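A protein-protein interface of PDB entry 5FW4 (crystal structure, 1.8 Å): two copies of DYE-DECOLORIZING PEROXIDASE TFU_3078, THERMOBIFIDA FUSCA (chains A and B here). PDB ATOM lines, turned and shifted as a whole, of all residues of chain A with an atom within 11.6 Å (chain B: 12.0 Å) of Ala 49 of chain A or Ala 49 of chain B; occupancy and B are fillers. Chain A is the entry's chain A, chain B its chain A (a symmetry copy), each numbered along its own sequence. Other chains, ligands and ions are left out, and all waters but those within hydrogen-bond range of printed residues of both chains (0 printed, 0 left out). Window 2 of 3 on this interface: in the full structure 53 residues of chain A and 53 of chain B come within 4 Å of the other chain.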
ATOM      1  N   ALA A  49     -20.015  22.275  23.345  1.00  0.00           N
ATOM      2  CA  ALA A  49     -19.012  22.420  22.262  1.00  0.00           C
ATOM      3  C   ALA A  49     -19.408  21.575  21.046  1.00  0.00           C
ATOM      4  O   ALA A  49     -20.281  20.707  21.153  1.00  0.00           O
ATOM      5  CB  ALA A  49     -17.625  22.033  22.749  1.00  0.00           C
ATOM      6  N   SER A  50     -18.750  21.852  19.924  1.00  0.00           N
ATOM      7  CA  SER A  50     -18.886  21.090  18.696  1.00  0.00           C
ATOM      8  C   SER A  50     -17.937  21.713  17.675  1.00  0.00           C
ATOM      9  O   SER A  50     -17.515  22.865  17.853  1.00  0.00           O
ATOM     10  CB  SER A  50     -20.339  21.119  18.170  1.00  0.00           C
ATOM     11  OG  SER A  50     -20.702  22.400  17.715  1.00  0.00           O
ATOM     12  N   PRO A  51     -17.574  20.963  16.618  1.00  0.00           N
ATOM     13  CA  PRO A  51     -16.841  21.531  15.520  1.00  0.00           C
ATOM     14  C   PRO A  51     -17.490  22.760  14.916  1.00  0.00           C
ATOM     15  O   PRO A  51     -16.829  23.763  14.718  1.00  0.00           O
ATOM     16  CB  PRO A  51     -16.812  20.390  14.512  1.00  0.00           C
ATOM     17  CG  PRO A  51     -16.690  19.201  15.380  1.00  0.00           C
ATOM     18  CD  PRO A  51     -17.452  19.497  16.631  1.00  0.00           C
ATOM     19  N   LYS A  52     -18.778  22.688  14.615  1.00  0.00           N
ATOM     20  CA  LYS A  52     -19.470  23.855  14.099  1.00  0.00           C
ATOM     21  C   LYS A  52     -19.351  25.062  15.043  1.00  0.00           C
ATOM     22  O   LYS A  52     -19.136  26.174  14.588  1.00  0.00           O
ATOM     23  CB  LYS A  52     -20.932  23.512  13.891  1.00  0.00           C
ATOM     24  CG  LYS A  52     -21.154  22.627  12.686  1.00  0.00           C
ATOM     25  CD  LYS A  52     -21.399  23.461  11.440  1.00  0.00           C
ATOM     26  CE  LYS A  52     -20.156  23.789  10.626  1.00  0.00           C
ATOM     27  NZ  LYS A  52     -19.732  22.693   9.691  1.00  0.00           N
ATOM     28  N   ALA A  53     -19.521  24.848  16.344  1.00  0.00           N
ATOM     29  CA  ALA A  53     -19.387  25.963  17.285  1.00  0.00           C
ATOM     30  C   ALA A  53     -17.997  26.582  17.215  1.00  0.00           C
ATOM     31  O   ALA A  53     -17.909  27.791  17.160  1.00  0.00           O
ATOM     32  CB  ALA A  53     -19.720  25.539  18.707  1.00  0.00           C
ATOM     33  N   GLU A  54     -16.929  25.778  17.201  1.00  0.00           N
ATOM     34  CA  GLU A  54     -15.576  26.337  17.072  1.00  0.00           C
ATOM     35  C   GLU A  54     -15.445  27.132  15.765  1.00  0.00           C
ATOM     36  O   GLU A  54     -14.838  28.212  15.714  1.00  0.00           O
ATOM     37  CB  GLU A  54     -14.496  25.257  17.204  1.00  0.00           C
ATOM     38  CG  GLU A  54     -14.173  24.889  18.649  1.00  0.00           C
ATOM     39  CD  GLU A  54     -13.180  23.748  18.779  1.00  0.00           C
ATOM     40  OE1 GLU A  54     -12.369  23.556  17.855  1.00  0.00           O
ATOM     41  OE2 GLU A  54     -13.222  23.029  19.815  1.00  0.00           O
ATOM     42  N   GLN A  55     -16.101  26.628  14.718  1.00  0.00           N
ATOM     43  CA  GLN A  55     -16.099  27.260  13.439  1.00  0.00           C
ATOM     44  C   GLN A  55     -16.862  28.606  13.448  1.00  0.00           C
ATOM     45  O   GLN A  55     -16.424  29.549  12.827  1.00  0.00           O
ATOM     46  CB  GLN A  55     -16.671  26.306  12.376  1.00  0.00           C
ATOM     47  CG  GLN A  55     -15.713  25.180  11.984  1.00  0.00           C
ATOM     48  CD  GLN A  55     -16.406  24.025  11.278  1.00  0.00           C
ATOM     49  OE1 GLN A  55     -17.334  24.230  10.499  1.00  0.00           O
ATOM     50  NE2 GLN A  55     -15.950  22.812  11.539  1.00  0.00           N
ATOM     51  N   ARG A  56     -17.981  28.679  14.173  1.00  0.00           N
ATOM     52  CA  ARG A  56     -18.743  29.898  14.345  1.00  0.00           C
ATOM     53  C   ARG A  56     -17.901  31.001  15.048  1.00  0.00           C
ATOM     54  O   ARG A  56     -18.129  32.191  14.838  1.00  0.00           O
ATOM     55  CB  ARG A  56     -19.990  29.634  15.172  1.00  0.00           C
ATOM     56  CG  ARG A  56     -21.105  28.904  14.434  1.00  0.00           C
ATOM     57  CD  ARG A  56     -22.385  28.762  15.255  1.00  0.00           C
ATOM     58  NE  ARG A  56     -23.181  27.724  14.580  1.00  0.00           N
ATOM     59  CZ  ARG A  56     -23.512  26.544  15.090  1.00  0.00           C
ATOM     60  NH1 ARG A  56     -23.256  26.248  16.357  1.00  0.00           N
ATOM     61  NH2 ARG A  56     -24.166  25.664  14.332  1.00  0.00           N
ATOM     62  N   LEU A  57     -16.958  30.602  15.872  1.00  0.00           N
ATOM     63  CA  LEU A  57     -16.128  31.589  16.643  1.00  0.00           C
ATOM     64  C   LEU A  57     -14.843  32.058  15.958  1.00  0.00           C
ATOM     65  O   LEU A  57     -14.196  33.048  16.416  1.00  0.00           O
ATOM     66  CB  LEU A  57     -15.764  31.040  18.015  1.00  0.00           C
ATOM     67  CG  LEU A  57     -16.890  31.051  19.051  1.00  0.00           C
ATOM     68  CD1 LEU A  57     -16.512  30.182  20.224  1.00  0.00           C
ATOM     69  CD2 LEU A  57     -17.270  32.476  19.483  1.00  0.00           C
ATOM     70  N   ARG A  58     -14.473  31.395  14.870  1.00  0.00           N
ATOM     71  CA  ARG A  58     -13.132  31.566  14.302  1.00  0.00           C
ATOM     72  C   ARG A  58     -12.884  32.974  13.746  1.00  0.00           C
ATOM     73  O   ARG A  58     -11.817  33.547  13.952  1.00  0.00           O
ATOM     74  CB  ARG A  58     -12.906  30.551  13.202  1.00  0.00           C
ATOM     75  CG  ARG A  58     -11.485  30.555  12.661  1.00  0.00           C
ATOM     76  CD  ARG A  58     -11.239  29.493  11.601  1.00  0.00           C
ATOM     77  NE  ARG A  58     -10.966  30.102  10.302  1.00  0.00           N
ATOM     78  CZ  ARG A  58     -11.887  30.561   9.451  1.00  0.00           C
ATOM     79  NH1 ARG A  58     -13.191  30.499   9.717  1.00  0.00           N
ATOM     80  NH2 ARG A  58     -11.497  31.095   8.303  1.00  0.00           N
ATOM     81  N   ALA A  61     -12.178  35.289  16.478  1.00  0.00           N
ATOM     82  CA  ALA A  61     -11.017  34.910  17.275  1.00  0.00           C
ATOM     83  C   ALA A  61      -9.688  35.179  16.578  1.00  0.00           C
ATOM     84  O   ALA A  61      -8.676  35.376  17.229  1.00  0.00           O
ATOM     85  CB  ALA A  61     -11.098  33.422  17.622  1.00  0.00           C
ATOM     86  N   ALA B  49     -12.359  24.142  22.005  1.00  0.00           N
ATOM     87  CA  ALA B  49     -13.503  24.443  22.901  1.00  0.00           C
ATOM     88  C   ALA B  49     -13.006  24.969  24.251  1.00  0.00           C
ATOM     89  O   ALA B  49     -11.817  24.845  24.565  1.00  0.00           O
ATOM     90  CB  ALA B  49     -14.376  23.214  23.098  1.00  0.00           C
ATOM     91  N   SER B  50     -13.934  25.541  25.014  1.00  0.00           N
ATOM     92  CA  SER B  50     -13.700  25.992  26.373  1.00  0.00           C
ATOM     93  C   SER B  50     -15.023  26.546  26.896  1.00  0.00           C
ATOM     94  O   SER B  50     -15.913  26.866  26.094  1.00  0.00           O
ATOM     95  CB  SER B  50     -12.601  27.078  26.427  1.00  0.00           C
ATOM     96  OG  SER B  50     -13.028  28.280  25.830  1.00  0.00           O
ATOM     97  N   PRO B  51     -15.179  26.644  28.229  1.00  0.00           N
ATOM     98  CA  PRO B  51     -16.309  27.325  28.797  1.00  0.00           C
ATOM     99  C   PRO B  51     -16.501  28.738  28.283  1.00  0.00           C
ATOM    100  O   PRO B  51     -17.597  29.103  27.901  1.00  0.00           O
ATOM    101  CB  PRO B  51     -15.979  27.337  30.284  1.00  0.00           C
ATOM    102  CG  PRO B  51     -15.308  26.034  30.472  1.00  0.00           C
ATOM    103  CD  PRO B  51     -14.550  25.751  29.215  1.00  0.00           C
ATOM    104  N   LYS B  52     -15.444  29.537  28.276  1.00  0.00           N
ATOM    105  CA  LYS B  52     -15.549  30.877  27.729  1.00  0.00           C
ATOM    106  C   LYS B  52     -16.050  30.871  26.277  1.00  0.00           C
ATOM    107  O   LYS B  52     -16.879  31.690  25.913  1.00  0.00           O
ATOM    108  CB  LYS B  52     -14.191  31.548  27.798  1.00  0.00           C
ATOM    109  CG  LYS B  52     -13.819  31.959  29.205  1.00  0.00           C
ATOM    110  CD  LYS B  52     -14.289  33.373  29.498  1.00  0.00           C
ATOM    111  CE  LYS B  52     -15.669  33.478  30.128  1.00  0.00           C
ATOM    112  NZ  LYS B  52     -15.679  33.271  31.615  1.00  0.00           N
ATOM    113  N   ALA B  53     -15.527  29.975  25.446  1.00  0.00           N
ATOM    114  CA  ALA B  53     -15.995  29.912  24.059  1.00  0.00           C
ATOM    115  C   ALA B  53     -17.488  29.616  23.993  1.00  0.00           C
ATOM    116  O   ALA B  53     -18.174  30.287  23.251  1.00  0.00           O
ATOM    117  CB  ALA B  53     -15.205  28.898  23.246  1.00  0.00           C
ATOM    118  N   GLU B  54     -17.991  28.642  24.760  1.00  0.00           N
ATOM    119  CA  GLU B  54     -19.435  28.369  24.768  1.00  0.00           C
ATOM    120  C   GLU B  54     -20.215  29.615  25.209  1.00  0.00           C
ATOM    121  O   GLU B  54     -21.274  29.954  24.659  1.00  0.00           O
ATOM    122  CB  GLU B  54     -19.780  27.139  25.614  1.00  0.00           C
ATOM    123  CG  GLU B  54     -19.565  25.816  24.885  1.00  0.00           C
ATOM    124  CD  GLU B  54     -19.807  24.596  25.756  1.00  0.00           C
ATOM    125  OE1 GLU B  54     -20.589  24.696  26.718  1.00  0.00           O
ATOM    126  OE2 GLU B  54     -19.196  23.528  25.477  1.00  0.00           O
ATOM    127  N   GLN B  55     -19.633  30.351  26.159  1.00  0.00           N
ATOM    128  CA  GLN B  55     -20.218  31.551  26.661  1.00  0.00           C
ATOM    129  C   GLN B  55     -20.242  32.680  25.604  1.00  0.00           C
ATOM    130  O   GLN B  55     -21.210  33.404  25.519  1.00  0.00           O
ATOM    131  CB  GLN B  55     -19.486  32.003  27.937  1.00  0.00           C
ATOM    132  CG  GLN B  55     -19.815  31.154  29.166  1.00  0.00           C
ATOM    133  CD  GLN B  55     -18.807  31.317  30.292  1.00  0.00           C
ATOM    134  OE1 GLN B  55     -18.292  32.408  30.523  1.00  0.00           O
ATOM    135  NE2 GLN B  55     -18.534  30.236  31.003  1.00  0.00           N
ATOM    136  N   ARG B  56     -19.184  32.797  24.798  1.00  0.00           N
ATOM    137  CA  ARG B  56     -19.112  33.747  23.708  1.00  0.00           C
ATOM    138  C   ARG B  56     -20.220  33.483  22.649  1.00  0.00           C
ATOM    139  O   ARG B  56     -20.664  34.404  21.965  1.00  0.00           O
ATOM    140  CB  ARG B  56     -17.757  33.671  23.024  1.00  0.00           C
ATOM    141  CG  ARG B  56     -16.611  34.303  23.804  1.00  0.00           C
ATOM    142  CD  ARG B  56     -15.289  34.316  23.038  1.00  0.00           C
ATOM    143  NE  ARG B  56     -14.245  34.576  24.043  1.00  0.00           N
ATOM    144  CZ  ARG B  56     -13.274  33.739  24.386  1.00  0.00           C
ATOM    145  NH1 ARG B  56     -13.074  32.608  23.725  1.00  0.00           N
ATOM    146  NH2 ARG B  56     -12.445  34.072  25.377  1.00  0.00           N
ATOM    147  N   LEU B  57     -20.642  32.246  22.518  1.00  0.00           N
ATOM    148  CA  LEU B  57     -21.670  31.877  21.485  1.00  0.00           C
ATOM    149  C   LEU B  57     -23.129  31.955  21.939  1.00  0.00           C
ATOM    150  O   LEU B  57     -24.069  31.887  21.090  1.00  0.00           O
ATOM    151  CB  LEU B  57     -21.415  30.480  20.937  1.00  0.00           C
ATOM    152  CG  LEU B  57     -20.254  30.360  19.948  1.00  0.00           C
ATOM    153  CD1 LEU B  57     -19.893  28.909  19.758  1.00  0.00           C
ATOM    154  CD2 LEU B  57     -20.551  31.063  18.614  1.00  0.00           C
ATOM    155  N   ARG B  58     -23.340  32.119  23.238  1.00  0.00           N
ATOM    156  CA  ARG B  58     -24.674  31.925  23.816  1.00  0.00           C
ATOM    157  C   ARG B  58     -25.699  32.961  23.337  1.00  0.00           C
ATOM    158  O   ARG B  58     -26.839  32.616  23.034  1.00  0.00           O
ATOM    159  CB  ARG B  58     -24.591  31.970  25.327  1.00  0.00           C
ATOM    160  CG  ARG B  58     -25.904  31.625  26.013  1.00  0.00           C
ATOM    161  CD  ARG B  58     -25.806  31.607  27.530  1.00  0.00           C
ATOM    162  NE  ARG B  58     -26.612  32.672  28.119  1.00  0.00           N
ATOM    163  CZ  ARG B  58     -26.244  33.951  28.234  1.00  0.00           C
ATOM    164  NH1 ARG B  58     -25.059  34.388  27.809  1.00  0.00           N
ATOM    165  NH2 ARG B  58     -27.079  34.817  28.789  1.00  0.00           N
ATOM    166  N   ALA B  61     -26.869  32.103  19.988  1.00  0.00           N
ATOM    167  CA  ALA B  61     -27.490  30.785  19.909  1.00  0.00           C
ATOM    168  C   ALA B  61     -28.889  30.737  20.512  1.00  0.00           C
ATOM    169  O   ALA B  61     -29.702  29.914  20.126  1.00  0.00           O
ATOM    170  CB  ALA B  61     -26.609  29.760  20.627  1.00  0.00           C
ATOM    171  N   GLN B  62     -29.153  31.546  21.519  1.00  0.00           N
ATOM    172  CA  GLN B  62     -30.417  31.385  22.270  1.00  0.00           C
ATOM    173  C   GLN B  62     -31.540  32.325  21.843  1.00  0.00           C
ATOM    174  O   GLN B  62     -31.283  33.408  21.317  1.00  0.00           O
ATOM    175  CB  GLN B  62     -30.155  31.586  23.750  1.00  0.00           C
ATOM    176  CG  GLN B  62     -29.339  30.459  24.343  1.00  0.00           C
ATOM    177  CD  GLN B  62     -29.069  30.680  25.812  1.00  0.00           C
ATOM    178  OE1 GLN B  62     -29.340  31.764  26.356  1.00  0.00           O
ATOM    179  NE2 GLN B  62     -28.501  29.661  26.466  1.00  0.00           N
ATOM    180  N   LEU B 136     -29.186  31.564  13.525  1.00  0.00           N
ATOM    181  CA  LEU B 136     -29.621  31.172  14.865  1.00  0.00           C
ATOM    182  C   LEU B 136     -30.525  32.258  15.452  1.00  0.00           C
ATOM    183  O   LEU B 136     -30.625  33.330  14.900  1.00  0.00           O
ATOM    184  CB  LEU B 136     -28.364  30.935  15.759  1.00  0.00           C
ATOM    185  CG  LEU B 136     -27.503  29.737  15.340  1.00  0.00           C
ATOM    186  CD1 LEU B 136     -26.204  29.705  16.142  1.00  0.00           C
ATOM    187  CD2 LEU B 136     -28.271  28.426  15.459  1.00  0.00           C
ATOM    188  N   ARG B 228     -13.184  38.864  24.856  1.00  0.00           N
ATOM    189  CA  ARG B 228     -12.320  37.972  25.604  1.00  0.00           C
ATOM    190  C   ARG B 228     -13.088  37.437  26.794  1.00  0.00           C
ATOM    191  O   ARG B 228     -12.957  36.285  27.133  1.00  0.00           O
ATOM    192  CB  ARG B 228     -11.048  38.691  26.123  1.00  0.00           C
ATOM    193  CG  ARG B 228     -10.114  39.106  25.014  1.00  0.00           C
ATOM    194  CD  ARG B 228      -8.682  39.385  25.467  1.00  0.00           C
ATOM    195  NE  ARG B 228      -7.957  39.588  24.226  1.00  0.00           N
ATOM    196  CZ  ARG B 228      -7.344  38.640  23.528  1.00  0.00           C
ATOM    197  NH1 ARG B 228      -7.268  37.402  23.999  1.00  0.00           N
ATOM    198  NH2 ARG B 228      -6.767  38.945  22.355  1.00  0.00           N
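The backbone NH of Ala 53 of chain A lies within hydrogen-bond range of the side-chain hydroxyl of Ser 50 of chain A (3.0 Å). O of Arg 228 of chain B is in hydrogen-bond range of NH2 of Arg 56 of chain B, 2.9 Å away. The side-chain hydroxyl (OG) of Ser 50 of chain B sits at hydrogen-bond distance from the backbone NH (N) of Ala 53 of chain B, 3.0 Å away.
The backbone NH (N) of Ala 49 of chain A lies within hydrogen-bond range of the side-chain carboxylate (OE2) of Glu 54 of chain B (2.6 Å). OE2 of Glu 54 of chain A is in hydrogen-bond range of N of Ala 49 of chain B (2.6 Å).
Of the 14 printed residues of chain B, 6 touch a printed residue of chain A. Hydrophobic or aromatic side chains of chain B that line the printed part of chain A: Ala 49, Ala 53, Leu 57 and Leu 136. Of the 11 printed residues of chain A, 5 touch a printed residue of chain B. Printed residues of chain A that touch a printed residue of chain B: Ala 49, Ala 53, Glu 54, Arg 56 and Leu 57. Hydrophobic or aromatic side chains of chain A that line the printed part of chain B: Ala 49, Ala 53 and Leu 57. Among the printed residues, no Asp or Glu carboxylate lies within 4 Å of a Lys or Arg side-chain nitrogen of the other chain.
Ala 49 of chain A touches its own counterpart, Ala 49 of chain B. Ala 49 of chain A touches Glu 54 of chain B, and with the chains exchanged Glu 54 of chain A touches Ala 49 of chain B. Arg 56 of chain A touches Leu 57 of chain B, and with the chains exchanged Leu 57 of chain A touches Arg 56 of chain B. Leu 57 of chain A touches its own counterpart, Leu 57 of chain B. Of the 9 pairs that touch across the chains among the printed residues, 8 have their exchanged pair printed and touching as well.
CB of Ala 49 of chain A touches CB of Ala 49 of chain B, at 3.5 Å. Ala 53 of chain A touches Leu 57 of chain B (O to CD1, 3.5 Å). Arg 56 of chain A touches Leu 57 of chain B. Leu 136 of chain B touches Arg 56 of chain A. Leu 57 of chain A touches Ala 53 of chain B (CD1 to O, 3.5 Å). Arg 56 of chain B touches Leu 57 of chain A. Leu 57 of chain A touches Leu 57 of chain B.
Ala 49 of chain A touches just these residues of chain B: Ala 49 (3.5 Å) and Glu 54 (2.6 Å). Of chain A, only Ala 49 (3.5 Å) and Glu 54 (2.6 Å) come within 4 Å of Ala 49 of chain B. Ser 50 of chain A touches none of the printed residues of chain B. No residue of chain B comes within 4 Å of Pro 51 of chain A. No residue of chain A comes within 4 Å of Ser 50 of chain B. No residue of chain A comes within 4 Å of Pro 51 of chain B. Of the printed residues of chain A, Leu 57 of chain B touches Ala 53, Arg 56 and Leu 57. Printed residues of chain A within 4 Å of Leu 136 of chain B: Arg 56. Lys 52 of chain B touches none of the printed residues of chain A. The nearest residue of chain B that does not touch Ala 49 of chain A is Ser 50 of chain B (5.6 Å).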
